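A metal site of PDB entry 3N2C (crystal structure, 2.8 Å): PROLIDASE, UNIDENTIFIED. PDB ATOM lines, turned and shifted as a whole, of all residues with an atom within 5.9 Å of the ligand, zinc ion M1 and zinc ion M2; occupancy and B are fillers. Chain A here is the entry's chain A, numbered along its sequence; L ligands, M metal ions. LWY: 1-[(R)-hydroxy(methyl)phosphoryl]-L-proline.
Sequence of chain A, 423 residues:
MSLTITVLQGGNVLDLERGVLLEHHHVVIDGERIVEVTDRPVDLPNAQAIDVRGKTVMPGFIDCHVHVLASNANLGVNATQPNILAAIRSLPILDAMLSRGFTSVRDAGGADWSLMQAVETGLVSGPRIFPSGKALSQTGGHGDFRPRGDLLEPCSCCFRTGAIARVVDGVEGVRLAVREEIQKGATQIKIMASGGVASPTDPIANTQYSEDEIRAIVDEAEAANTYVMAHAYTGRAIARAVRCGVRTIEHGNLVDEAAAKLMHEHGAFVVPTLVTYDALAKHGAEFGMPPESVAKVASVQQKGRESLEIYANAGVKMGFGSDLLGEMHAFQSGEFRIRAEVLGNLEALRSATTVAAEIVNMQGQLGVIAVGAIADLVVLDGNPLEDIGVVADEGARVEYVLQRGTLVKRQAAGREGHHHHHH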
ATOM      1  N   HIS A  65     -18.722  -4.450   8.844  1.00  0.00           N
ATOM      2  CA  HIS A  65     -18.258  -5.574   9.639  1.00  0.00           C
ATOM      3  C   HIS A  65     -16.830  -5.982   9.301  1.00  0.00           C
ATOM      4  O   HIS A  65     -16.581  -6.729   8.348  1.00  0.00           O
ATOM      5  CB  HIS A  65     -19.219  -6.766   9.465  1.00  0.00           C
ATOM      6  CG  HIS A  65     -19.113  -7.783  10.566  1.00  0.00           C
ATOM      7  ND1 HIS A  65     -20.096  -7.942  11.527  1.00  0.00           N
ATOM      8  CD2 HIS A  65     -18.150  -8.672  10.862  1.00  0.00           C
ATOM      9  CE1 HIS A  65     -19.734  -8.909  12.361  1.00  0.00           C
ATOM     10  NE2 HIS A  65     -18.553  -9.372  11.974  1.00  0.00           N
ATOM     11  N   VAL A  66     -15.879  -5.487  10.084  1.00  0.00           N
ATOM     12  CA  VAL A  66     -14.479  -5.888   9.940  1.00  0.00           C
ATOM     13  C   VAL A  66     -13.878  -6.398  11.250  1.00  0.00           C
ATOM     14  O   VAL A  66     -14.424  -6.194  12.340  1.00  0.00           O
ATOM     15  CB  VAL A  66     -13.573  -4.754   9.374  1.00  0.00           C
ATOM     16  CG1 VAL A  66     -14.041  -4.318   8.017  1.00  0.00           C
ATOM     17  CG2 VAL A  66     -13.521  -3.575  10.317  1.00  0.00           C
ATOM     18  N   HIS A  67     -12.741  -7.084  11.130  1.00  0.00           N
ATOM     19  CA  HIS A  67     -11.906  -7.416  12.271  1.00  0.00           C
ATOM     20  C   HIS A  67     -10.483  -7.026  11.940  1.00  0.00           C
ATOM     21  O   HIS A  67      -9.678  -7.844  11.494  1.00  0.00           O
ATOM     22  CB  HIS A  67     -12.006  -8.891  12.615  1.00  0.00           C
ATOM     23  CG  HIS A  67     -13.288  -9.274  13.262  1.00  0.00           C
ATOM     24  ND1 HIS A  67     -13.715  -8.710  14.451  1.00  0.00           N
ATOM     25  CD2 HIS A  67     -14.237 -10.153  12.902  1.00  0.00           C
ATOM     26  CE1 HIS A  67     -14.887  -9.227  14.785  1.00  0.00           C
ATOM     27  NE2 HIS A  67     -15.219 -10.119  13.858  1.00  0.00           N
ATOM     28  N   LEU A  75      -8.661 -17.352  15.365  1.00  0.00           N
ATOM     29  CA  LEU A  75      -8.992 -16.329  16.357  1.00  0.00           C
ATOM     30  C   LEU A  75      -8.607 -16.728  17.778  1.00  0.00           C
ATOM     31  O   LEU A  75      -8.480 -15.871  18.654  1.00  0.00           O
ATOM     32  CB  LEU A  75     -10.475 -15.970  16.302  1.00  0.00           C
ATOM     33  CG  LEU A  75     -11.040 -15.335  15.030  1.00  0.00           C
ATOM     34  CD1 LEU A  75     -12.533 -15.150  15.180  1.00  0.00           C
ATOM     35  CD2 LEU A  75     -10.369 -14.007  14.715  1.00  0.00           C
ATOM     36  N   ALA A 108     -15.925  -4.976  14.435  1.00  0.00           N
ATOM     37  CA  ALA A 108     -16.895  -5.821  15.117  1.00  0.00           C
ATOM     38  C   ALA A 108     -16.316  -6.536  16.331  1.00  0.00           C
ATOM     39  O   ALA A 108     -16.930  -7.457  16.856  1.00  0.00           O
ATOM     40  CB  ALA A 108     -17.477  -6.823  14.139  1.00  0.00           C
ATOM     41  N   HIS A 142     -19.445 -17.760  21.591  1.00  0.00           N
ATOM     42  CA  HIS A 142     -18.715 -17.586  20.339  1.00  0.00           C
ATOM     43  C   HIS A 142     -17.388 -16.844  20.526  1.00  0.00           C
ATOM     44  O   HIS A 142     -16.469 -16.984  19.707  1.00  0.00           O
ATOM     45  CB  HIS A 142     -19.603 -16.887  19.296  1.00  0.00           C
ATOM     46  CG  HIS A 142     -19.027 -16.892  17.909  1.00  0.00           C
ATOM     47  ND1 HIS A 142     -18.279 -17.946  17.421  1.00  0.00           N
ATOM     48  CD2 HIS A 142     -19.084 -15.983  16.910  1.00  0.00           C
ATOM     49  CE1 HIS A 142     -17.895 -17.670  16.184  1.00  0.00           C
ATOM     50  NE2 HIS A 142     -18.384 -16.501  15.849  1.00  0.00           N
ATOM     51  N   ILE A 164     -10.546 -10.572  20.071  1.00  0.00           N
ATOM     52  CA  ILE A 164     -11.780 -10.094  19.454  1.00  0.00           C
ATOM     53  C   ILE A 164     -12.869  -9.816  20.497  1.00  0.00           C
ATOM     54  O   ILE A 164     -13.547  -8.783  20.453  1.00  0.00           O
ATOM     55  CB  ILE A 164     -12.307 -11.126  18.406  1.00  0.00           C
ATOM     56  CG1 ILE A 164     -11.215 -11.474  17.377  1.00  0.00           C
ATOM     57  CG2 ILE A 164     -13.582 -10.652  17.729  1.00  0.00           C
ATOM     58  CD1 ILE A 164     -10.724 -10.300  16.529  1.00  0.00           C
ATOM     59  N   KCX A 190     -20.918  -4.748  20.608  1.00  0.00           N
ATOM     60  CA  KCX A 190     -21.071  -6.046  19.971  1.00  0.00           C
ATOM     61  CB  KCX A 190     -19.789  -6.447  19.247  1.00  0.00           C
ATOM     62  CG  KCX A 190     -19.831  -7.835  18.628  1.00  0.00           C
ATOM     63  CD  KCX A 190     -20.807  -7.888  17.457  1.00  0.00           C
ATOM     64  CE  KCX A 190     -20.690  -9.187  16.688  1.00  0.00           C
ATOM     65  NZ  KCX A 190     -19.374  -9.296  15.984  1.00  0.00           N
ATOM     66  C   KCX A 190     -21.457  -7.123  20.991  1.00  0.00           C
ATOM     67  O   KCX A 190     -20.917  -7.154  22.100  1.00  0.00           O
ATOM     68  CX  KCX A 190     -19.046 -10.413  15.359  1.00  0.00           C
ATOM     69  OQ1 KCX A 190     -19.826 -11.385  15.363  1.00  0.00           O
ATOM     70  OQ2 KCX A 190     -17.962 -10.508  14.766  1.00  0.00           O
ATOM     71  N   MET A 192     -22.502 -11.620  21.107  1.00  0.00           N
ATOM     72  CA  MET A 192     -22.694 -12.917  20.448  1.00  0.00           C
ATOM     73  C   MET A 192     -24.036 -13.492  20.903  1.00  0.00           C
ATOM     74  O   MET A 192     -24.160 -14.003  22.020  1.00  0.00           O
ATOM     75  CB  MET A 192     -21.555 -13.880  20.798  1.00  0.00           C
ATOM     76  CG  MET A 192     -20.154 -13.344  20.556  1.00  0.00           C
ATOM     77  SD  MET A 192     -19.779 -13.063  18.825  1.00  0.00           S
ATOM     78  CE  MET A 192     -18.013 -12.770  18.898  1.00  0.00           C
ATOM     79  N   GLY A 195     -24.595 -19.236  18.366  1.00  0.00           N
ATOM     80  CA  GLY A 195     -23.402 -19.984  18.026  1.00  0.00           C
ATOM     81  C   GLY A 195     -22.769 -19.475  16.746  1.00  0.00           C
ATOM     82  O   GLY A 195     -23.450 -18.872  15.905  1.00  0.00           O
ATOM     83  N   GLY A 196     -21.473 -19.695  16.594  1.00  0.00           N
ATOM     84  CA  GLY A 196     -20.763 -19.264  15.408  1.00  0.00           C
ATOM     85  C   GLY A 196     -19.897 -20.361  14.819  1.00  0.00           C
ATOM     86  O   GLY A 196     -19.919 -21.507  15.268  1.00  0.00           O
ATOM     87  N   VAL A 197     -19.122 -19.976  13.804  1.00  0.00           N
ATOM     88  CA  VAL A 197     -18.330 -20.924  13.006  1.00  0.00           C
ATOM     89  C   VAL A 197     -16.893 -21.055  13.539  1.00  0.00           C
ATOM     90  O   VAL A 197     -16.336 -22.153  13.560  1.00  0.00           O
ATOM     91  CB  VAL A 197     -18.312 -20.510  11.515  1.00  0.00           C
ATOM     92  CG1 VAL A 197     -17.760 -21.603  10.660  1.00  0.00           C
ATOM     93  CG2 VAL A 197     -19.716 -20.145  11.042  1.00  0.00           C
ATOM     94  N   ALA A 198     -16.332 -19.940  13.997  1.00  0.00           N
ATOM     95  CA  ALA A 198     -14.924 -19.862  14.436  1.00  0.00           C
ATOM     96  C   ALA A 198     -14.636 -20.561  15.767  1.00  0.00           C
ATOM     97  O   ALA A 198     -13.625 -21.264  15.889  1.00  0.00           O
ATOM     98  CB  ALA A 198     -14.454 -18.408  14.468  1.00  0.00           C
ATOM     99  N   SER A 199     -15.497 -20.349  16.752  1.00  0.00           N
ATOM    100  CA  SER A 199     -15.357 -20.963  18.083  1.00  0.00           C
ATOM    101  C   SER A 199     -15.609 -22.471  18.049  1.00  0.00           C
ATOM    102  O   SER A 199     -16.560 -22.921  17.395  1.00  0.00           O
ATOM    103  CB  SER A 199     -16.322 -20.293  19.072  1.00  0.00           C
ATOM    104  OG  SER A 199     -17.637 -20.277  18.546  1.00  0.00           O
ATOM    105  N   ILE A 204     -23.837 -23.617  15.485  1.00  0.00           N
ATOM    106  CA  ILE A 204     -24.478 -22.393  14.975  1.00  0.00           C
ATOM    107  C   ILE A 204     -25.994 -22.348  15.204  1.00  0.00           C
ATOM    108  O   ILE A 204     -26.609 -21.268  15.143  1.00  0.00           O
ATOM    109  CB  ILE A 204     -24.177 -22.184  13.457  1.00  0.00           C
ATOM    110  CG1 ILE A 204     -24.653 -23.382  12.628  1.00  0.00           C
ATOM    111  CG2 ILE A 204     -22.696 -21.923  13.230  1.00  0.00           C
ATOM    112  CD1 ILE A 204     -24.975 -23.060  11.205  1.00  0.00           C
ATOM    113  N   HIS A 231     -24.357 -10.774  16.598  1.00  0.00           N
ATOM    114  CA  HIS A 231     -24.048 -11.941  15.780  1.00  0.00           C
ATOM    115  C   HIS A 231     -25.101 -13.039  16.003  1.00  0.00           C
ATOM    116  O   HIS A 231     -25.258 -13.554  17.108  1.00  0.00           O
ATOM    117  CB  HIS A 231     -22.627 -12.415  16.124  1.00  0.00           C
ATOM    118  CG  HIS A 231     -22.352 -13.847  15.827  1.00  0.00           C
ATOM    119  ND1 HIS A 231     -21.852 -14.268  14.613  1.00  0.00           N
ATOM    120  CD2 HIS A 231     -22.470 -14.970  16.585  1.00  0.00           C
ATOM    121  CE1 HIS A 231     -21.689 -15.576  14.634  1.00  0.00           C
ATOM    122  NE2 HIS A 231     -22.061 -16.027  15.816  1.00  0.00           N
ATOM    123  N   TYR A 233     -27.271 -16.376  13.593  1.00  0.00           N
ATOM    124  CA  TYR A 233     -27.437 -17.124  12.336  1.00  0.00           C
ATOM    125  C   TYR A 233     -28.880 -17.537  12.058  1.00  0.00           C
ATOM    126  O   TYR A 233     -29.449 -17.154  11.034  1.00  0.00           O
ATOM    127  CB  TYR A 233     -26.528 -18.350  12.308  1.00  0.00           C
ATOM    128  CG  TYR A 233     -25.107 -18.025  11.927  1.00  0.00           C
ATOM    129  CD1 TYR A 233     -24.817 -17.493  10.681  1.00  0.00           C
ATOM    130  CD2 TYR A 233     -24.065 -18.247  12.814  1.00  0.00           C
ATOM    131  CE1 TYR A 233     -23.519 -17.196  10.314  1.00  0.00           C
ATOM    132  CE2 TYR A 233     -22.747 -17.945  12.457  1.00  0.00           C
ATOM    133  CZ  TYR A 233     -22.485 -17.415  11.207  1.00  0.00           C
ATOM    134  OH  TYR A 233     -21.200 -17.109  10.834  1.00  0.00           O
ATOM    135  N   GLU A 250     -25.722  -9.282  12.471  1.00  0.00           N
ATOM    136  CA  GLU A 250     -24.595  -9.691  11.630  1.00  0.00           C
ATOM    137  C   GLU A 250     -24.889 -11.048  11.010  1.00  0.00           C
ATOM    138  O   GLU A 250     -25.632 -11.850  11.586  1.00  0.00           O
ATOM    139  CB  GLU A 250     -23.299  -9.713  12.444  1.00  0.00           C
ATOM    140  CG  GLU A 250     -23.100  -8.514  13.357  1.00  0.00           C
ATOM    141  CD  GLU A 250     -23.165  -7.184  12.627  1.00  0.00           C
ATOM    142  OE1 GLU A 250     -22.550  -7.045  11.550  1.00  0.00           O
ATOM    143  OE2 GLU A 250     -23.836  -6.261  13.138  1.00  0.00           O
ATOM    144  N   HIS A 251     -24.293 -11.286   9.842  1.00  0.00           N
ATOM    145  CA  HIS A 251     -24.415 -12.544   9.069  1.00  0.00           C
ATOM    146  C   HIS A 251     -25.851 -12.874   8.655  1.00  0.00           C
ATOM    147  O   HIS A 251     -26.233 -12.664   7.504  1.00  0.00           O
ATOM    148  CB  HIS A 251     -23.751 -13.719   9.795  1.00  0.00           C
ATOM    149  CG  HIS A 251     -22.477 -13.349  10.484  1.00  0.00           C
ATOM    150  ND1 HIS A 251     -21.274 -13.256   9.822  1.00  0.00           N
ATOM    151  CD2 HIS A 251     -22.223 -13.031  11.776  1.00  0.00           C
ATOM    152  CE1 HIS A 251     -20.332 -12.890  10.682  1.00  0.00           C
ATOM    153  NE2 HIS A 251     -20.889 -12.751  11.875  1.00  0.00           N
ATOM    154  N   THR A 273     -22.353 -11.084   5.576  1.00  0.00           N
ATOM    155  CA  THR A 273     -20.929 -11.074   5.222  1.00  0.00           C
ATOM    156  C   THR A 273     -20.613 -12.335   4.438  1.00  0.00           C
ATOM    157  O   THR A 273     -20.043 -13.280   4.964  1.00  0.00           O
ATOM    158  CB  THR A 273     -20.024 -11.005   6.483  1.00  0.00           C
ATOM    159  OG1 THR A 273     -20.306 -12.118   7.341  1.00  0.00           O
ATOM    160  CG2 THR A 273     -20.235  -9.721   7.267  1.00  0.00           C
ATOM    161  N   THR A 276     -16.723 -14.078   3.261  1.00  0.00           N
ATOM    162  CA  THR A 276     -15.845 -14.805   4.190  1.00  0.00           C
ATOM    163  C   THR A 276     -16.002 -16.326   4.099  1.00  0.00           C
ATOM    164  O   THR A 276     -15.022 -17.052   4.243  1.00  0.00           O
ATOM    165  CB  THR A 276     -15.937 -14.265   5.648  1.00  0.00           C
ATOM    166  OG1 THR A 276     -14.991 -14.957   6.479  1.00  0.00           O
ATOM    167  CG2 THR A 276     -17.327 -14.413   6.238  1.00  0.00           C
ATOM    168  N   TYR A 277     -17.229 -16.786   3.832  1.00  0.00           N
ATOM    169  CA  TYR A 277     -17.515 -18.208   3.746  1.00  0.00           C
ATOM    170  C   TYR A 277     -16.984 -18.805   2.450  1.00  0.00           C
ATOM    171  O   TYR A 277     -16.532 -19.955   2.428  1.00  0.00           O
ATOM    172  CB  TYR A 277     -19.020 -18.446   3.874  1.00  0.00           C
ATOM    173  CG  TYR A 277     -19.634 -17.791   5.077  1.00  0.00           C
ATOM    174  CD1 TYR A 277     -19.384 -18.268   6.368  1.00  0.00           C
ATOM    175  CD2 TYR A 277     -20.455 -16.672   4.932  1.00  0.00           C
ATOM    176  CE1 TYR A 277     -19.933 -17.651   7.481  1.00  0.00           C
ATOM    177  CE2 TYR A 277     -21.018 -16.055   6.044  1.00  0.00           C
ATOM    178  CZ  TYR A 277     -20.757 -16.550   7.321  1.00  0.00           C
ATOM    179  OH  TYR A 277     -21.310 -15.941   8.414  1.00  0.00           O
ATOM    180  N   LEU A 280     -13.309 -19.093   3.065  1.00  0.00           N
ATOM    181  CA  LEU A 280     -13.069 -20.249   3.944  1.00  0.00           C
ATOM    182  C   LEU A 280     -13.483 -21.584   3.302  1.00  0.00           C
ATOM    183  O   LEU A 280     -13.224 -22.649   3.858  1.00  0.00           O
ATOM    184  CB  LEU A 280     -13.766 -20.063   5.296  1.00  0.00           C
ATOM    185  CG  LEU A 280     -13.248 -18.953   6.224  1.00  0.00           C
ATOM    186  CD1 LEU A 280     -14.194 -18.747   7.400  1.00  0.00           C
ATOM    187  CD2 LEU A 280     -11.822 -19.222   6.691  1.00  0.00           C
ATOM    188  N   ASP A 323     -16.006  -9.335   6.986  1.00  0.00           N
ATOM    189  CA  ASP A 323     -15.683 -10.276   8.084  1.00  0.00           C
ATOM    190  C   ASP A 323     -14.519 -11.230   7.748  1.00  0.00           C
ATOM    191  O   ASP A 323     -14.504 -12.396   8.150  1.00  0.00           O
ATOM    192  CB  ASP A 323     -16.945 -11.036   8.514  1.00  0.00           C
ATOM    193  CG  ASP A 323     -16.810 -11.716   9.865  1.00  0.00           C
ATOM    194  OD1 ASP A 323     -16.270 -11.089  10.809  1.00  0.00           O
ATOM    195  OD2 ASP A 323     -17.243 -12.876   9.985  1.00  0.00           O
ATOM    196  N   LEU A 325     -10.605 -12.689   7.738  1.00  0.00           N
ATOM    197  CA  LEU A 325      -9.563 -12.856   8.750  1.00  0.00           C
ATOM    198  C   LEU A 325      -8.213 -13.139   8.096  1.00  0.00           C
ATOM    199  O   LEU A 325      -8.126 -13.903   7.130  1.00  0.00           O
ATOM    200  CB  LEU A 325      -9.922 -14.002   9.711  1.00  0.00           C
ATOM    201  CG  LEU A 325     -11.358 -14.176  10.188  1.00  0.00           C
ATOM    202  CD1 LEU A 325     -11.563 -15.577  10.731  1.00  0.00           C
ATOM    203  CD2 LEU A 325     -11.781 -13.136  11.219  1.00  0.00           C
HETATM  204  C   LWY L   1     -18.386 -16.932  12.568  1.00  0.00           C
HETATM  205  N   LWY L   1     -16.784 -15.142  12.025  1.00  0.00           N
HETATM  206  OXT LWY L   1     -19.584 -17.176  12.804  1.00  0.00           O
HETATM  207  P   LWY L   1     -16.694 -14.085  13.316  1.00  0.00           P
HETATM  208  C1  LWY L   1     -15.109 -13.414  13.382  1.00  0.00           C
HETATM  209  O1  LWY L   1     -16.883 -14.934  14.660  1.00  0.00           O
HETATM  210  O2  LWY L   1     -17.649 -12.951  13.056  1.00  0.00           O
HETATM  211  CA  LWY L   1     -18.040 -15.792  11.647  1.00  0.00           C
HETATM  212  CB  LWY L   1     -17.771 -16.308  10.240  1.00  0.00           C
HETATM  213  CD  LWY L   1     -15.646 -15.498  11.179  1.00  0.00           C
HETATM  214  CG  LWY L   1     -16.290 -16.146   9.962  1.00  0.00           C
HETATM  215  O   LWY L   1     -17.462 -17.589  13.077  1.00  0.00           O
HETATM  216 ZN    ZN M   1     -17.171 -10.668  12.991  1.00  0.00          ZN
HETATM  217 ZN    ZN M   2     -19.704 -13.157  14.228  1.00  0.00          ZN
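OH of Tyr 233 lies within hydrogen-bond range of OXT of the ligand.
NE2 of His 142 sits at hydrogen-bond distance from O1 of the ligand, 2.5 Å away.
An oxygen (O) of the ligand is in hydrogen-bond range of the backbone NH of Ala 198.
The backbone NH (N) of Val 197 lies within hydrogen-bond range of an oxygen (O) of the ligand (3.0 Å).
NE2 of His 231 lies within hydrogen-bond range of O of Gly 195 (3.2 Å).
A ring nitrogen (ND1) of His 65 sits at hydrogen-bond distance from the side-chain carboxylate (OE1) of Glu 250, at 2.6 Å.
The side-chain hydroxyl (OH) of Tyr 233 is in hydrogen-bond range of the side-chain hydroxyl (OH) of Tyr 277 (2.7 Å).
NZ of KCX 190 sits at hydrogen-bond distance from the backbone carbonyl oxygen of Ala 108 (3.2 Å).
A ring nitrogen (ND1) of His 251 lies within hydrogen-bond range of the side-chain hydroxyl (OG1) of Thr 273 (2.9 Å).
O of Asp 323 sits at hydrogen-bond distance from OG1 of Thr 276 (3.1 Å).
The side-chain hydroxyl (OH) of Tyr 277 is in hydrogen-bond range of a ring nitrogen (ND1) of His 251 (3.0 Å).
The side-chain hydroxyl of Ser 199 sits at hydrogen-bond distance from a ring nitrogen (ND1) of His 142, 2.7 Å away.
CD1 of Leu 75 touches C1 of the ligand, at 3.6 Å.
Gly 196 touches the ligand (CA to OXT, 3.5 Å).
Thr 276 touches the ligand (OG1 to CG, 3.9 Å).
CE1 of Tyr 277 touches CB of the ligand, at 3.8 Å.
Leu 325 touches the ligand (CD2 to C1, 3.98 Å).
Hydrophobic or aromatic side chains that line the ligand: His 67, Leu 75, His 142, Val 197, Ala 198, His 231, Tyr 233, His 251, Tyr 277 and Leu 325.
Within 4 Å of the ligand: His 65, His 67, Leu 75, His 142, KCX 190, Gly 196, Val 197, Ala 198, His 231, Tyr 233, His 251, Thr 276, Tyr 277, Asp 323 and Leu 325.
The nearest printed residue that does not touch zinc ion M1 is Ala 108 (4.02 Å).
Residues that only touch zinc ion M2: His 142 (3.9 Å).
Within 4 Å of zinc ion M2: His 142, KCX 190, His 231 and His 251.
The nearest printed residue that does not touch zinc ion M2 is His 65 (4.6 Å).
Zinc ion M1 is bound by OQ2 of KCX 190, at 1.9 Å.
NE2 of His 65 binds zinc ion M1, 2.2 Å away.
NE2 of His 67 is bound to zinc ion M1 (2.2 Å).
Zinc ion M1 is bound by O2 of the ligand (2.3 Å).
OD1 of Asp 323 binds zinc ion M1, at 2.4 Å.
Zinc ion M1 has five donor atoms within binding distance.
Zinc ion M2 is bound by OQ1 of KCX 190 (2.1 Å), an oxygen (O2) of the ligand (2.4 Å), a ring nitrogen (ND1) of His 231 (2.4 Å) and a ring nitrogen (NE2) of His 251 (2.7 Å).
Zinc ion M2 has four donor atoms within binding distance.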
